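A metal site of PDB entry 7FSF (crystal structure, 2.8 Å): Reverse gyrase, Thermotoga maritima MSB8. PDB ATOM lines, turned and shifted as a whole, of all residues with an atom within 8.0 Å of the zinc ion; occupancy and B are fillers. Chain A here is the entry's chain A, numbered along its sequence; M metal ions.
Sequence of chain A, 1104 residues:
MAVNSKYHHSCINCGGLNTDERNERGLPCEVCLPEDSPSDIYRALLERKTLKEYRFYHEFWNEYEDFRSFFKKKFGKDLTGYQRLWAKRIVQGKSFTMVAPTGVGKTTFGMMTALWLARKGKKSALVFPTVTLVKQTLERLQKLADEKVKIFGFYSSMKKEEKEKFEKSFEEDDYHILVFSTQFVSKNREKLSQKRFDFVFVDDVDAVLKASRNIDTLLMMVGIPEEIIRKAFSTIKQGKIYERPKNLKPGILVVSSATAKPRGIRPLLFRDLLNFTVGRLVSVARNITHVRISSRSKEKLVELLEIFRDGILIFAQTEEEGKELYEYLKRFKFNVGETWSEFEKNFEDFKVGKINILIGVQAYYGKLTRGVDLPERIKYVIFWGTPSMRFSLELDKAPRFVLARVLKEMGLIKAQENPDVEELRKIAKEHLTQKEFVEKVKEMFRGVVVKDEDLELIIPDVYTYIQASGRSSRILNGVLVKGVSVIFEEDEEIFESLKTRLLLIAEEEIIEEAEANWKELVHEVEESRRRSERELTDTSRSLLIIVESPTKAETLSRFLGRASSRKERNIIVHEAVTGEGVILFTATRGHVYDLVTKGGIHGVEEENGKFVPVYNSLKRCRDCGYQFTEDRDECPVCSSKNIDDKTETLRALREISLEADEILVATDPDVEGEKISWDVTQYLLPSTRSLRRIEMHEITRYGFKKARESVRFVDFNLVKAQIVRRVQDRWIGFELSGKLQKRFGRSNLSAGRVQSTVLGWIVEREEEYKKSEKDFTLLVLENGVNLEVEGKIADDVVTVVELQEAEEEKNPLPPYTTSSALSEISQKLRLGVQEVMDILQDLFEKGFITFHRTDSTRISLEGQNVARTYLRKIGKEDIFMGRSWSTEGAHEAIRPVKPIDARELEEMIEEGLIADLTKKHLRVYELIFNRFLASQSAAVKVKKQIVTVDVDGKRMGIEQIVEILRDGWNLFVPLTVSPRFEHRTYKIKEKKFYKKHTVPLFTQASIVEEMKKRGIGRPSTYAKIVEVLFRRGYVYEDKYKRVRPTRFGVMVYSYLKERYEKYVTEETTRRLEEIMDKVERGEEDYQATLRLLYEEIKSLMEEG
The zinc ion is bound by SG of Cys 29 (2.2 Å), SG of Cys 14 (2.2 Å), SG of Cys 32 (2.3 Å) and SG of Cys 11 (2.3 Å).
The zinc ion has four donor atoms within binding distance.
The backbone carbonyl oxygen (O) of Gly 16 is in hydrogen-bond range of the backbone NH (N) of Cys 11, 3.0 Å away.
SG of Cys 32 lies close to NZ of Lys 52, at 3.3 Å.
OG1 of Thr 50 is in hydrogen-bond range of O of Cys 32 (2.9 Å).
SG of Cys 14 lies close to N of Gly 16, 3.6 Å away.
The backbone NH of Val 31 lies close to the side-chain sulfur of Cys 29 (3.5 Å).
N of Asn 13 lies close to SG of Cys 11 (3.5 Å).
The side-chain amide nitrogen (ND2) of Asn 13 lies close to the side-chain sulfur (SG) of Cys 32.
Within 4 Å of the zinc ion: Cys 11, Cys 14, Cys 29 and Cys 32.
The nearest printed residue that does not touch the zinc ion is Asn 13 (4.5 Å).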
ATOM      1  N   SER A  10     -16.072 -18.750   6.740  1.00  0.00           N
ATOM      2  CA  SER A  10     -15.107 -18.505   7.808  1.00  0.00           C
ATOM      3  C   SER A  10     -13.969 -17.577   7.410  1.00  0.00           C
ATOM      4  O   SER A  10     -13.438 -16.875   8.277  1.00  0.00           O
ATOM      5  CB  SER A  10     -14.532 -19.835   8.310  1.00  0.00           C
ATOM      6  OG  SER A  10     -14.085 -20.634   7.237  1.00  0.00           O
ATOM      7  N   CYS A  11     -13.552 -17.584   6.144  1.00  0.00           N
ATOM      8  CA  CYS A  11     -12.405 -16.779   5.741  1.00  0.00           C
ATOM      9  C   CYS A  11     -12.632 -15.321   6.096  1.00  0.00           C
ATOM     10  O   CYS A  11     -13.675 -14.751   5.768  1.00  0.00           O
ATOM     11  CB  CYS A  11     -12.125 -16.934   4.251  1.00  0.00           C
ATOM     12  SG  CYS A  11     -10.689 -15.972   3.665  1.00  0.00           S
ATOM     13  N   ILE A  12     -11.657 -14.711   6.770  1.00  0.00           N
ATOM     14  CA  ILE A  12     -11.828 -13.337   7.225  1.00  0.00           C
ATOM     15  C   ILE A  12     -11.629 -12.333   6.097  1.00  0.00           C
ATOM     16  O   ILE A  12     -12.090 -11.190   6.207  1.00  0.00           O
ATOM     17  CB  ILE A  12     -10.862 -13.054   8.397  1.00  0.00           C
ATOM     18  CG1 ILE A  12     -11.240 -11.759   9.110  1.00  0.00           C
ATOM     19  CG2 ILE A  12      -9.430 -13.010   7.903  1.00  0.00           C
ATOM     20  CD1 ILE A  12     -10.472 -11.511  10.386  1.00  0.00           C
ATOM     21  N   ASN A  13     -10.989 -12.730   5.004  1.00  0.00           N
ATOM     22  CA  ASN A  13     -10.710 -11.808   3.907  1.00  0.00           C
ATOM     23  C   ASN A  13     -11.833 -11.776   2.867  1.00  0.00           C
ATOM     24  O   ASN A  13     -12.320 -10.700   2.508  1.00  0.00           O
ATOM     25  CB  ASN A  13      -9.384 -12.182   3.232  1.00  0.00           C
ATOM     26  CG  ASN A  13      -8.890 -11.117   2.273  1.00  0.00           C
ATOM     27  OD1 ASN A  13      -9.140  -9.927   2.485  1.00  0.00           O
ATOM     28  ND2 ASN A  13      -8.206 -11.540   1.217  1.00  0.00           N
ATOM     29  N   CYS A  14     -12.250 -12.950   2.375  1.00  0.00           N
ATOM     30  CA  CYS A  14     -13.261 -13.030   1.335  1.00  0.00           C
ATOM     31  C   CYS A  14     -14.616 -13.507   1.844  1.00  0.00           C
ATOM     32  O   CYS A  14     -15.542 -13.679   1.045  1.00  0.00           O
ATOM     33  CB  CYS A  14     -12.792 -13.957   0.207  1.00  0.00           C
ATOM     34  SG  CYS A  14     -12.681 -15.718   0.637  1.00  0.00           S
ATOM     35  N   GLY A  15     -14.754 -13.740   3.153  1.00  0.00           N
ATOM     36  CA  GLY A  15     -16.028 -14.164   3.705  1.00  0.00           C
ATOM     37  C   GLY A  15     -16.539 -15.477   3.178  1.00  0.00           C
ATOM     38  O   GLY A  15     -17.730 -15.769   3.314  1.00  0.00           O
ATOM     39  N   GLY A  16     -15.673 -16.297   2.575  1.00  0.00           N
ATOM     40  CA  GLY A  16     -16.060 -17.552   1.986  1.00  0.00           C
ATOM     41  C   GLY A  16     -15.530 -18.751   2.746  1.00  0.00           C
ATOM     42  O   GLY A  16     -15.182 -18.673   3.938  1.00  0.00           O
ATOM     43  N   LEU A  17     -15.483 -19.890   2.057  1.00  0.00           N
ATOM     44  CA  LEU A  17     -15.075 -21.139   2.674  1.00  0.00           C
ATOM     45  C   LEU A  17     -13.597 -21.085   3.079  1.00  0.00           C
ATOM     46  O   LEU A  17     -12.769 -20.477   2.404  1.00  0.00           O
ATOM     47  CB  LEU A  17     -15.327 -22.306   1.726  1.00  0.00           C
ATOM     48  CG  LEU A  17     -15.332 -23.711   2.318  1.00  0.00           C
ATOM     49  CD1 LEU A  17     -16.413 -24.568   1.696  1.00  0.00           C
ATOM     50  CD2 LEU A  17     -13.979 -24.366   2.136  1.00  0.00           C
ATOM     51  N   ASN A  18     -13.299 -21.720   4.208  1.00  0.00           N
ATOM     52  CA  ASN A  18     -11.929 -21.796   4.722  1.00  0.00           C
ATOM     53  C   ASN A  18     -11.876 -22.931   5.723  1.00  0.00           C
ATOM     54  O   ASN A  18     -12.876 -23.254   6.371  1.00  0.00           O
ATOM     55  CB  ASN A  18     -11.487 -20.477   5.365  1.00  0.00           C
ATOM     56  CG  ASN A  18     -10.010 -20.453   5.714  1.00  0.00           C
ATOM     57  OD1 ASN A  18      -9.223 -21.263   5.205  1.00  0.00           O
ATOM     58  ND2 ASN A  18      -9.620 -19.540   6.593  1.00  0.00           N
ATOM     59  N   LEU A  27      -5.063 -17.383   9.581  1.00  0.00           N
ATOM     60  CA  LEU A  27      -4.841 -17.195   8.156  1.00  0.00           C
ATOM     61  C   LEU A  27      -6.166 -17.128   7.393  1.00  0.00           C
ATOM     62  O   LEU A  27      -7.153 -17.737   7.796  1.00  0.00           O
ATOM     63  CB  LEU A  27      -4.008 -18.354   7.601  1.00  0.00           C
ATOM     64  CG  LEU A  27      -2.632 -18.559   8.227  1.00  0.00           C
ATOM     65  CD1 LEU A  27      -2.052 -19.888   7.777  1.00  0.00           C
ATOM     66  CD2 LEU A  27      -1.712 -17.420   7.832  1.00  0.00           C
ATOM     67  N   PRO A  28      -6.200 -16.383   6.292  1.00  0.00           N
ATOM     68  CA  PRO A  28      -7.348 -16.455   5.388  1.00  0.00           C
ATOM     69  C   PRO A  28      -7.244 -17.699   4.519  1.00  0.00           C
ATOM     70  O   PRO A  28      -6.291 -18.481   4.614  1.00  0.00           O
ATOM     71  CB  PRO A  28      -7.232 -15.171   4.548  1.00  0.00           C
ATOM     72  CG  PRO A  28      -6.033 -14.420   5.094  1.00  0.00           C
ATOM     73  CD  PRO A  28      -5.200 -15.429   5.815  1.00  0.00           C
ATOM     74  N   CYS A  29      -8.231 -17.867   3.640  1.00  0.00           N
ATOM     75  CA  CYS A  29      -8.379 -19.120   2.920  1.00  0.00           C
ATOM     76  C   CYS A  29      -7.235 -19.341   1.930  1.00  0.00           C
ATOM     77  O   CYS A  29      -6.442 -18.443   1.632  1.00  0.00           O
ATOM     78  CB  CYS A  29      -9.721 -19.162   2.187  1.00  0.00           C
ATOM     79  SG  CYS A  29      -9.853 -18.023   0.803  1.00  0.00           S
ATOM     80  N   GLU A  30      -7.151 -20.573   1.441  1.00  0.00           N
ATOM     81  CA  GLU A  30      -6.121 -20.949   0.469  1.00  0.00           C
ATOM     82  C   GLU A  30      -6.229 -20.149  -0.821  1.00  0.00           C
ATOM     83  O   GLU A  30      -5.224 -19.945  -1.508  1.00  0.00           O
ATOM     84  CB  GLU A  30      -6.223 -22.445   0.182  1.00  0.00           C
ATOM     85  CG  GLU A  30      -7.598 -22.931  -0.330  1.00  0.00           C
ATOM     86  CD  GLU A  30      -8.675 -22.963   0.753  1.00  0.00           C
ATOM     87  OE1 GLU A  30      -8.348 -22.867   1.950  1.00  0.00           O
ATOM     88  OE2 GLU A  30      -9.870 -23.092   0.389  1.00  0.00           O
ATOM     89  N   VAL A  31      -7.436 -19.693  -1.172  1.00  0.00           N
ATOM     90  CA  VAL A  31      -7.598 -18.892  -2.379  1.00  0.00           C
ATOM     91  C   VAL A  31      -7.035 -17.488  -2.181  1.00  0.00           C
ATOM     92  O   VAL A  31      -6.335 -16.960  -3.044  1.00  0.00           O
ATOM     93  CB  VAL A  31      -9.081 -18.836  -2.793  1.00  0.00           C
ATOM     94  CG1 VAL A  31      -9.234 -18.083  -4.107  1.00  0.00           C
ATOM     95  CG2 VAL A  31      -9.646 -20.235  -2.896  1.00  0.00           C
ATOM     96  N   CYS A  32      -7.340 -16.866  -1.038  1.00  0.00           N
ATOM     97  CA  CYS A  32      -6.856 -15.520  -0.779  1.00  0.00           C
ATOM     98  C   CYS A  32      -5.342 -15.501  -0.570  1.00  0.00           C
ATOM     99  O   CYS A  32      -4.681 -14.534  -0.959  1.00  0.00           O
ATOM    100  CB  CYS A  32      -7.550 -14.934   0.458  1.00  0.00           C
ATOM    101  SG  CYS A  32      -9.290 -14.502   0.244  1.00  0.00           S
ATOM    102  N   LEU A  33      -4.785 -16.545   0.048  1.00  0.00           N
ATOM    103  CA  LEU A  33      -3.373 -16.542   0.426  1.00  0.00           C
ATOM    104  C   LEU A  33      -2.847 -17.962   0.377  1.00  0.00           C
ATOM    105  O   LEU A  33      -2.852 -18.684   1.387  1.00  0.00           O
ATOM    106  CB  LEU A  33      -3.188 -15.937   1.814  1.00  0.00           C
ATOM    107  CG  LEU A  33      -1.770 -15.720   2.343  1.00  0.00           C
ATOM    108  CD1 LEU A  33      -0.910 -15.014   1.312  1.00  0.00           C
ATOM    109  CD2 LEU A  33      -1.847 -14.929   3.631  1.00  0.00           C
ATOM    110  N   LEU A  45      -1.827 -10.370   1.212  1.00  0.00           N
ATOM    111  CA  LEU A  45      -3.048 -10.288   0.409  1.00  0.00           C
ATOM    112  C   LEU A  45      -2.975  -9.147  -0.590  1.00  0.00           C
ATOM    113  O   LEU A  45      -3.550  -9.246  -1.685  1.00  0.00           O
ATOM    114  CB  LEU A  45      -4.260 -10.104   1.315  1.00  0.00           C
ATOM    115  CG  LEU A  45      -4.495 -11.162   2.399  1.00  0.00           C
ATOM    116  CD1 LEU A  45      -5.499 -10.650   3.403  1.00  0.00           C
ATOM    117  CD2 LEU A  45      -4.978 -12.469   1.775  1.00  0.00           C
ATOM    118  N   THR A  50      -5.691  -9.722  -3.738  1.00  0.00           N
ATOM    119  CA  THR A  50      -6.889 -10.345  -3.198  1.00  0.00           C
ATOM    120  C   THR A  50      -7.318  -9.737  -1.864  1.00  0.00           C
ATOM    121  O   THR A  50      -8.194 -10.300  -1.188  1.00  0.00           O
ATOM    122  CB  THR A  50      -6.693 -11.849  -3.021  1.00  0.00           C
ATOM    123  OG1 THR A  50      -5.492 -12.087  -2.271  1.00  0.00           O
ATOM    124  CG2 THR A  50      -6.588 -12.528  -4.380  1.00  0.00           C
ATOM    125  N   LYS A  52      -9.425  -7.948   0.385  1.00  0.00           N
ATOM    126  CA  LYS A  52     -10.802  -7.489   0.280  1.00  0.00           C
ATOM    127  C   LYS A  52     -11.352  -6.928   1.583  1.00  0.00           C
ATOM    128  O   LYS A  52     -11.784  -5.775   1.620  1.00  0.00           O
ATOM    129  CB  LYS A  52     -11.684  -8.624  -0.228  1.00  0.00           C
ATOM    130  CG  LYS A  52     -11.185  -9.264  -1.511  1.00  0.00           C
ATOM    131  CD  LYS A  52     -12.108 -10.382  -1.976  1.00  0.00           C
ATOM    132  CE  LYS A  52     -11.356 -11.439  -2.753  1.00  0.00           C
ATOM    133  NZ  LYS A  52     -10.406 -12.203  -1.880  1.00  0.00           N
HETATM  134 ZN    ZN M   1     -10.580 -16.051   1.356  1.00  0.00          ZN
